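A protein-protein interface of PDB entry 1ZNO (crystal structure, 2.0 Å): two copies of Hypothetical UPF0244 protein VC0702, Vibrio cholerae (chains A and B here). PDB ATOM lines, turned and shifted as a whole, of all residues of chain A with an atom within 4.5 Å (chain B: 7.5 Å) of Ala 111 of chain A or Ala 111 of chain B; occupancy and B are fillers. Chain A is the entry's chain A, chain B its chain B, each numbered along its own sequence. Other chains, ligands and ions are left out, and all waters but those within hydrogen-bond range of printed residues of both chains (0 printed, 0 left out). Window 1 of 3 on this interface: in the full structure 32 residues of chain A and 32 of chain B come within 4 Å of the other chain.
Of chain B, only Arg 109 (3.0 Å), Ser 110 (3.9 Å), Ala 111 (3.8 Å) and Leu 169 (3.5 Å) come within 4 Å of Ala 111 of chain A. Of the printed residues of chain B, Leu 169 of chain A touches Ala 111 (3.5 Å), Cys 112 (3.8 Å), Leu 113 (3.6 Å) and Leu 157 (3.6 Å). Of the printed residues of chain A, Leu 113 of chain B touches Leu 169 (3.6 Å). The nearest residue of chain B that does not touch Ala 111 of chain A is Ser 108 of chain B (4.2 Å). The nearest residue of chain A that does not touch Ala 111 of chain B is Ser 108 of chain A (4.2 Å).
The backbone NH (N) of Ser 110 of chain B lies within hydrogen-bond range of the backbone carbonyl oxygen (O) of Ala 95 of chain B (2.9 Å). The guanidinium group of Arg 109 of chain B lies close to the side-chain sulfur of Cys 112 of chain B, 3.5 Å away. The backbone NH (N) of Met 97 of chain B is in hydrogen-bond range of the backbone carbonyl oxygen (O) of Ser 108 of chain B. The backbone NH (N) of Thr 93 of chain B sits at hydrogen-bond distance from the backbone carbonyl oxygen (O) of Leu 113 of chain B. The guanidinium group (NH2) of Arg 109 of chain A lies close to the side-chain sulfur (SG) of Cys 112 of chain A, 3.7 Å away. The backbone NH (N) of Thr 93 of chain A lies within hydrogen-bond range of the backbone carbonyl oxygen (O) of Leu 113 of chain A (2.9 Å).
Hydrophobic or aromatic side chains of chain A that line the printed part of chain B: Ala 111, Leu 113 and Leu 169. Hydrophobic or aromatic side chains of chain B that line the printed part of chain A: Ala 111, Leu 113, Leu 157 and Leu 169. Among the printed residues, no Asp or Glu carboxylate lies within 4 Å of a Lys or Arg side-chain nitrogen of the other chain.
Ser 108 of chain A touches Cys 112 of chain B, and with the chains exchanged Cys 112 of chain A touches Ser 108 of chain B. Arg 109 of chain A touches Ala 111 of chain B, and with the chains exchanged Ala 111 of chain A touches Arg 109 of chain B. Arg 109 of chain A touches Cys 112 of chain B, and with the chains exchanged Cys 112 of chain A touches Arg 109 of chain B. Ser 110 of chain A touches Ala 111 of chain B, and with the chains exchanged Ala 111 of chain A touches Ser 110 of chain B. Of the 17 pairs that touch across the chains among the printed residues, 16 have their exchanged pair printed and touching as well.
Among the printed residues, pairs that only touch across the chains: Ala 111 of chain A with Arg 109 of chain B, Arg 109 of chain A with Ala 111 of chain B, Ala 111 of chain A with Leu 169 of chain B, Leu 169 of chain A with Ala 111 of chain B, Leu 169 of chain A with Leu 157 of chain B, Arg 109 of chain A with Arg 109 of chain B, Leu 169 of chain A with Leu 113 of chain B, Leu 169 of chain A with Cys 112 of chain B, Ala 111 of chain A with Ala 111 of chain B, Cys 112 of chain A with Leu 169 of chain B, Ala 111 of chain A with Ser 110 of chain B, Ser 110 of chain A with Ala 111 of chain B and Leu 113 of chain A with Leu 169 of chain B.
O of Arg 109 of chain A sits at hydrogen-bond distance from N of Cys 112 of chain B (3.2 Å). The backbone carbonyl oxygen of Cys 112 of chain A lies within hydrogen-bond range of the side-chain hydroxyl of Ser 108 of chain B (2.7 Å). The backbone carbonyl oxygen (O) of Cys 112 of chain B lies within hydrogen-bond range of the side-chain hydroxyl (OG) of Ser 108 of chain A, 2.8 Å away. N of Cys 112 of chain A lies within hydrogen-bond range of O of Arg 109 of chain B, 3.2 Å away.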
ATOM      1  N   THR A  93     -14.498  23.296  30.149  1.00  0.00           N
ATOM      2  CA  THR A  93     -14.699  22.421  31.283  1.00  0.00           C
ATOM      3  C   THR A  93     -16.212  22.232  31.472  1.00  0.00           C
ATOM      4  O   THR A  93     -17.017  23.074  31.061  1.00  0.00           O
ATOM      5  CB  THR A  93     -14.041  22.977  32.571  1.00  0.00           C
ATOM      6  OG1 THR A  93     -13.878  21.904  33.505  1.00  0.00           O
ATOM      7  CG2 THR A  93     -14.899  24.068  33.217  1.00  0.00           C
ATOM      8  N   PHE A  94     -16.594  21.117  32.080  1.00  0.00           N
ATOM      9  CA  PHE A  94     -18.002  20.802  32.270  1.00  0.00           C
ATOM     10  C   PHE A  94     -18.076  19.557  33.146  1.00  0.00           C
ATOM     11  O   PHE A  94     -17.058  18.931  33.446  1.00  0.00           O
ATOM     12  CB  PHE A  94     -18.618  20.497  30.906  1.00  0.00           C
ATOM     13  CG  PHE A  94     -17.778  19.561  30.082  1.00  0.00           C
ATOM     14  CD1 PHE A  94     -17.723  18.200  30.383  1.00  0.00           C
ATOM     15  CD2 PHE A  94     -16.965  20.055  29.068  1.00  0.00           C
ATOM     16  CE1 PHE A  94     -16.855  17.346  29.692  1.00  0.00           C
ATOM     17  CE2 PHE A  94     -16.097  19.216  28.374  1.00  0.00           C
ATOM     18  CZ  PHE A  94     -16.041  17.859  28.685  1.00  0.00           C
ATOM     19  N   SER A 108     -27.469  14.275  31.984  1.00  0.00           N
ATOM     20  CA  SER A 108     -27.356  15.644  31.508  1.00  0.00           C
ATOM     21  C   SER A 108     -25.942  16.120  31.754  1.00  0.00           C
ATOM     22  O   SER A 108     -25.335  15.784  32.777  1.00  0.00           O
ATOM     23  CB  SER A 108     -28.306  16.557  32.286  1.00  0.00           C
ATOM     24  OG  SER A 108     -27.980  17.929  32.071  1.00  0.00           O
ATOM     25  N   ARG A 109     -25.415  16.900  30.818  1.00  0.00           N
ATOM     26  CA  ARG A 109     -24.081  17.467  30.974  1.00  0.00           C
ATOM     27  C   ARG A 109     -24.302  18.962  31.224  1.00  0.00           C
ATOM     28  O   ARG A 109     -25.055  19.615  30.502  1.00  0.00           O
ATOM     29  CB  ARG A 109     -23.261  17.285  29.696  1.00  0.00           C
ATOM     30  CG  ARG A 109     -21.770  17.540  29.886  1.00  0.00           C
ATOM     31  CD  ARG A 109     -21.078  17.932  28.581  1.00  0.00           C
ATOM     32  NE  ARG A 109     -21.303  19.348  28.285  1.00  0.00           N
ATOM     33  CZ  ARG A 109     -20.793  19.991  27.239  1.00  0.00           C
ATOM     34  NH1 ARG A 109     -20.023  19.346  26.375  1.00  0.00           N
ATOM     35  NH2 ARG A 109     -21.050  21.282  27.068  1.00  0.00           N
ATOM     36  N   SER A 110     -23.640  19.503  32.237  1.00  0.00           N
ATOM     37  CA  SER A 110     -23.786  20.911  32.575  1.00  0.00           C
ATOM     38  C   SER A 110     -23.318  21.835  31.458  1.00  0.00           C
ATOM     39  O   SER A 110     -22.616  21.408  30.532  1.00  0.00           O
ATOM     40  CB  SER A 110     -22.974  21.223  33.827  1.00  0.00           C
ATOM     41  OG  SER A 110     -21.602  21.022  33.545  1.00  0.00           O
ATOM     42  N   ALA A 111     -23.704  23.105  31.547  1.00  0.00           N
ATOM     43  CA  ALA A 111     -23.266  24.083  30.558  1.00  0.00           C
ATOM     44  C   ALA A 111     -21.735  24.128  30.651  1.00  0.00           C
ATOM     45  O   ALA A 111     -21.167  23.988  31.737  1.00  0.00           O
ATOM     46  CB  ALA A 111     -23.851  25.459  30.882  1.00  0.00           C
ATOM     47  N   CYS A 112     -21.058  24.322  29.528  1.00  0.00           N
ATOM     48  CA  CYS A 112     -19.601  24.358  29.562  1.00  0.00           C
ATOM     49  C   CYS A 112     -19.059  25.776  29.667  1.00  0.00           C
ATOM     50  O   CYS A 112     -19.721  26.749  29.289  1.00  0.00           O
ATOM     51  CB  CYS A 112     -19.009  23.670  28.329  1.00  0.00           C
ATOM     52  SG  CYS A 112     -19.343  24.526  26.780  1.00  0.00           S
ATOM     53  N   LEU A 113     -17.835  25.870  30.176  1.00  0.00           N
ATOM     54  CA  LEU A 113     -17.155  27.136  30.378  1.00  0.00           C
ATOM     55  C   LEU A 113     -15.746  27.134  29.786  1.00  0.00           C
ATOM     56  O   LEU A 113     -15.046  26.120  29.820  1.00  0.00           O
ATOM     57  CB  LEU A 113     -17.100  27.427  31.879  1.00  0.00           C
ATOM     58  CG  LEU A 113     -16.000  28.327  32.444  1.00  0.00           C
ATOM     59  CD1 LEU A 113     -16.544  29.146  33.601  1.00  0.00           C
ATOM     60  CD2 LEU A 113     -14.833  27.471  32.899  1.00  0.00           C
ATOM     61  N   LEU A 169     -32.109  18.413  35.342  1.00  0.00           N
ATOM     62  CA  LEU A 169     -32.307  17.921  33.983  1.00  0.00           C
ATOM     63  C   LEU A 169     -32.073  16.423  33.901  1.00  0.00           C
ATOM     64  O   LEU A 169     -32.726  15.725  33.128  1.00  0.00           O
ATOM     65  CB  LEU A 169     -31.357  18.633  33.018  1.00  0.00           C
ATOM     66  CG  LEU A 169     -31.650  20.121  32.853  1.00  0.00           C
ATOM     67  CD1 LEU A 169     -30.597  20.741  31.954  1.00  0.00           C
ATOM     68  CD2 LEU A 169     -33.051  20.307  32.255  1.00  0.00           C
ATOM     69  N   THR B  93     -31.148  17.743  23.607  1.00  0.00           N
ATOM     70  CA  THR B  93     -31.387  19.080  23.085  1.00  0.00           C
ATOM     71  C   THR B  93     -30.560  20.052  23.935  1.00  0.00           C
ATOM     72  O   THR B  93     -30.235  19.771  25.090  1.00  0.00           O
ATOM     73  CB  THR B  93     -32.889  19.452  23.111  1.00  0.00           C
ATOM     74  OG1 THR B  93     -33.085  20.656  22.361  1.00  0.00           O
ATOM     75  CG2 THR B  93     -33.387  19.647  24.542  1.00  0.00           C
ATOM     76  N   PHE B  94     -30.216  21.192  23.351  1.00  0.00           N
ATOM     77  CA  PHE B  94     -29.368  22.163  24.023  1.00  0.00           C
ATOM     78  C   PHE B  94     -29.314  23.403  23.145  1.00  0.00           C
ATOM     79  O   PHE B  94     -29.882  23.412  22.059  1.00  0.00           O
ATOM     80  CB  PHE B  94     -27.957  21.578  24.138  1.00  0.00           C
ATOM     81  CG  PHE B  94     -27.479  20.933  22.862  1.00  0.00           C
ATOM     82  CD1 PHE B  94     -27.015  21.712  21.800  1.00  0.00           C
ATOM     83  CD2 PHE B  94     -27.571  19.552  22.688  1.00  0.00           C
ATOM     84  CE1 PHE B  94     -26.659  21.128  20.586  1.00  0.00           C
ATOM     85  CE2 PHE B  94     -27.218  18.961  21.477  1.00  0.00           C
ATOM     86  CZ  PHE B  94     -26.761  19.748  20.419  1.00  0.00           C
ATOM     87  N   ALA B  95     -28.620  24.436  23.602  1.00  0.00           N
ATOM     88  CA  ALA B  95     -28.498  25.643  22.806  1.00  0.00           C
ATOM     89  C   ALA B  95     -27.086  26.181  22.907  1.00  0.00           C
ATOM     90  O   ALA B  95     -26.439  26.072  23.952  1.00  0.00           O
ATOM     91  CB  ALA B  95     -29.492  26.701  23.290  1.00  0.00           C
ATOM     92  N   MET B  97     -24.596  29.412  22.796  1.00  0.00           N
ATOM     93  CA  MET B  97     -24.562  30.846  23.058  1.00  0.00           C
ATOM     94  C   MET B  97     -23.238  31.374  22.527  1.00  0.00           C
ATOM     95  O   MET B  97     -22.177  30.862  22.899  1.00  0.00           O
ATOM     96  CB  MET B  97     -24.586  31.111  24.564  1.00  0.00           C
ATOM     97  CG  MET B  97     -25.867  31.652  25.130  1.00  0.00           C
ATOM     98  SD  MET B  97     -27.422  30.722  24.516  1.00  0.00           S
ATOM     99  CE  MET B  97     -26.896  28.953  25.030  1.00  0.00           C
ATOM    100  N   SER B 108     -20.588  29.369  25.060  1.00  0.00           N
ATOM    101  CA  SER B 108     -21.015  28.387  26.040  1.00  0.00           C
ATOM    102  C   SER B 108     -22.221  27.679  25.487  1.00  0.00           C
ATOM    103  O   SER B 108     -23.062  28.277  24.805  1.00  0.00           O
ATOM    104  CB  SER B 108     -21.394  29.050  27.371  1.00  0.00           C
ATOM    105  OG  SER B 108     -21.852  28.072  28.301  1.00  0.00           O
ATOM    106  N   ARG B 109     -22.285  26.390  25.772  1.00  0.00           N
ATOM    107  CA  ARG B 109     -23.404  25.570  25.357  1.00  0.00           C
ATOM    108  C   ARG B 109     -24.151  25.281  26.655  1.00  0.00           C
ATOM    109  O   ARG B 109     -23.542  24.929  27.666  1.00  0.00           O
ATOM    110  CB  ARG B 109     -22.925  24.252  24.752  1.00  0.00           C
ATOM    111  CG  ARG B 109     -23.980  23.572  23.897  1.00  0.00           C
ATOM    112  CD  ARG B 109     -23.825  22.064  23.922  1.00  0.00           C
ATOM    113  NE  ARG B 109     -24.249  21.570  25.227  1.00  0.00           N
ATOM    114  CZ  ARG B 109     -24.214  20.302  25.622  1.00  0.00           C
ATOM    115  NH1 ARG B 109     -23.761  19.356  24.804  1.00  0.00           N
ATOM    116  NH2 ARG B 109     -24.638  19.991  26.846  1.00  0.00           N
ATOM    117  N   SER B 110     -25.465  25.439  26.619  1.00  0.00           N
ATOM    118  CA  SER B 110     -26.296  25.202  27.783  1.00  0.00           C
ATOM    119  C   SER B 110     -26.281  23.731  28.155  1.00  0.00           C
ATOM    120  O   SER B 110     -25.818  22.883  27.378  1.00  0.00           O
ATOM    121  CB  SER B 110     -27.737  25.615  27.499  1.00  0.00           C
ATOM    122  OG  SER B 110     -28.278  24.814  26.466  1.00  0.00           O
ATOM    123  N   ALA B 111     -26.785  23.431  29.349  1.00  0.00           N
ATOM    124  CA  ALA B 111     -26.863  22.050  29.812  1.00  0.00           C
ATOM    125  C   ALA B 111     -27.804  21.316  28.866  1.00  0.00           C
ATOM    126  O   ALA B 111     -28.816  21.873  28.445  1.00  0.00           O
ATOM    127  CB  ALA B 111     -27.404  22.003  31.217  1.00  0.00           C
ATOM    128  N   CYS B 112     -27.478  20.073  28.524  1.00  0.00           N
ATOM    129  CA  CYS B 112     -28.335  19.316  27.614  1.00  0.00           C
ATOM    130  C   CYS B 112     -29.406  18.523  28.360  1.00  0.00           C
ATOM    131  O   CYS B 112     -29.256  18.199  29.543  1.00  0.00           O
ATOM    132  CB  CYS B 112     -27.507  18.392  26.699  1.00  0.00           C
ATOM    133  SG  CYS B 112     -26.494  17.159  27.540  1.00  0.00           S
ATOM    134  N   LEU B 113     -30.483  18.211  27.649  1.00  0.00           N
ATOM    135  CA  LEU B 113     -31.620  17.496  28.221  1.00  0.00           C
ATOM    136  C   LEU B 113     -32.151  16.377  27.315  1.00  0.00           C
ATOM    137  O   LEU B 113     -32.205  16.526  26.093  1.00  0.00           O
ATOM    138  CB  LEU B 113     -32.725  18.520  28.515  1.00  0.00           C
ATOM    139  CG  LEU B 113     -34.206  18.135  28.561  1.00  0.00           C
ATOM    140  CD1 LEU B 113     -34.975  19.157  29.377  1.00  0.00           C
ATOM    141  CD2 LEU B 113     -34.763  18.065  27.155  1.00  0.00           C
ATOM    142  N   ILE B 149     -38.176  22.564  28.435  1.00  0.00           N
ATOM    143  CA  ILE B 149     -37.496  22.453  29.725  1.00  0.00           C
ATOM    144  C   ILE B 149     -38.459  22.664  30.894  1.00  0.00           C
ATOM    145  O   ILE B 149     -38.499  21.867  31.835  1.00  0.00           O
ATOM    146  CB  ILE B 149     -36.356  23.480  29.832  1.00  0.00           C
ATOM    147  CG1 ILE B 149     -35.191  23.043  28.936  1.00  0.00           C
ATOM    148  CG2 ILE B 149     -35.923  23.639  31.295  1.00  0.00           C
ATOM    149  CD1 ILE B 149     -34.095  24.090  28.793  1.00  0.00           C
ATOM    150  N   LEU B 157     -37.157  24.306  36.268  1.00  0.00           N
ATOM    151  CA  LEU B 157     -36.223  24.977  35.390  1.00  0.00           C
ATOM    152  C   LEU B 157     -37.082  25.481  34.250  1.00  0.00           C
ATOM    153  O   LEU B 157     -38.192  24.994  34.043  1.00  0.00           O
ATOM    154  CB  LEU B 157     -35.166  24.015  34.838  1.00  0.00           C
ATOM    155  CG  LEU B 157     -34.093  23.483  35.789  1.00  0.00           C
ATOM    156  CD1 LEU B 157     -33.145  22.544  35.024  1.00  0.00           C
ATOM    157  CD2 LEU B 157     -33.308  24.646  36.386  1.00  0.00           C
ATOM    158  N   VAL B 162     -32.247  28.437  32.075  1.00  0.00           N
ATOM    159  CA  VAL B 162     -31.175  27.585  31.585  1.00  0.00           C
ATOM    160  C   VAL B 162     -30.324  28.423  30.634  1.00  0.00           C
ATOM    161  O   VAL B 162     -29.094  28.412  30.703  1.00  0.00           O
ATOM    162  CB  VAL B 162     -31.741  26.345  30.850  1.00  0.00           C
ATOM    163  CG1 VAL B 162     -30.618  25.556  30.186  1.00  0.00           C
ATOM    164  CG2 VAL B 162     -32.481  25.458  31.842  1.00  0.00           C
ATOM    165  N   TYR B 163     -30.976  29.162  29.747  1.00  0.00           N
ATOM    166  CA  TYR B 163     -30.247  30.016  28.809  1.00  0.00           C
ATOM    167  C   TYR B 163     -29.466  31.099  29.563  1.00  0.00           C
ATOM    168  O   TYR B 163     -28.369  31.478  29.152  1.00  0.00           O
ATOM    169  CB  TYR B 163     -31.220  30.678  27.838  1.00  0.00           C
ATOM    170  CG  TYR B 163     -31.701  29.783  26.714  1.00  0.00           C
ATOM    171  CD1 TYR B 163     -31.517  28.402  26.750  1.00  0.00           C
ATOM    172  CD2 TYR B 163     -32.369  30.327  25.623  1.00  0.00           C
ATOM    173  CE1 TYR B 163     -31.991  27.587  25.721  1.00  0.00           C
ATOM    174  CE2 TYR B 163     -32.846  29.532  24.595  1.00  0.00           C
ATOM    175  CZ  TYR B 163     -32.658  28.165  24.646  1.00  0.00           C
ATOM    176  OH  TYR B 163     -33.156  27.397  23.622  1.00  0.00           O
ATOM    177  N   GLN B 165     -27.881  30.975  32.400  1.00  0.00           N
ATOM    178  CA  GLN B 165     -26.588  30.480  32.863  1.00  0.00           C
ATOM    179  C   GLN B 165     -25.579  30.414  31.717  1.00  0.00           C
ATOM    180  O   GLN B 165     -24.459  30.899  31.842  1.00  0.00           O
ATOM    181  CB  GLN B 165     -26.729  29.091  33.503  1.00  0.00           C
ATOM    182  CG  GLN B 165     -27.690  29.045  34.686  1.00  0.00           C
ATOM    183  CD  GLN B 165     -27.242  28.095  35.782  1.00  0.00           C
ATOM    184  OE1 GLN B 165     -26.548  27.109  35.527  1.00  0.00           O
ATOM    185  NE2 GLN B 165     -27.654  28.379  37.010  1.00  0.00           N
ATOM    186  N   ALA B 166     -25.980  29.818  30.600  1.00  0.00           N
ATOM    187  CA  ALA B 166     -25.089  29.700  29.462  1.00  0.00           C
ATOM    188  C   ALA B 166     -24.647  31.082  28.993  1.00  0.00           C
ATOM    189  O   ALA B 166     -23.475  31.287  28.674  1.00  0.00           O
ATOM    190  CB  ALA B 166     -25.776  28.940  28.323  1.00  0.00           C
ATOM    191  N   LEU B 167     -25.575  32.031  28.950  1.00  0.00           N
ATOM    192  CA  LEU B 167     -25.225  33.383  28.514  1.00  0.00           C
ATOM    193  C   LEU B 167     -24.163  33.994  29.419  1.00  0.00           C
ATOM    194  O   LEU B 167     -23.195  34.587  28.943  1.00  0.00           O
ATOM    195  CB  LEU B 167     -26.472  34.277  28.469  1.00  0.00           C
ATOM    196  CG  LEU B 167     -27.277  34.077  27.181  1.00  0.00           C
ATOM    197  CD1 LEU B 167     -28.653  34.692  27.331  1.00  0.00           C
ATOM    198  CD2 LEU B 167     -26.526  34.704  25.994  1.00  0.00           C
ATOM    199  N   LEU B 169     -22.016  32.397  31.240  1.00  0.00           N
ATOM    200  CA  LEU B 169     -20.770  31.678  30.999  1.00  0.00           C
ATOM    201  C   LEU B 169     -20.094  32.194  29.726  1.00  0.00           C
ATOM    202  O   LEU B 169     -18.879  32.373  29.693  1.00  0.00           O
ATOM    203  CB  LEU B 169     -21.030  30.164  30.898  1.00  0.00           C
ATOM    204  CG  LEU B 169     -21.551  29.588  32.217  1.00  0.00           C
ATOM    205  CD1 LEU B 169     -21.946  28.113  32.097  1.00  0.00           C
ATOM    206  CD2 LEU B 169     -20.456  29.769  33.263  1.00  0.00           C
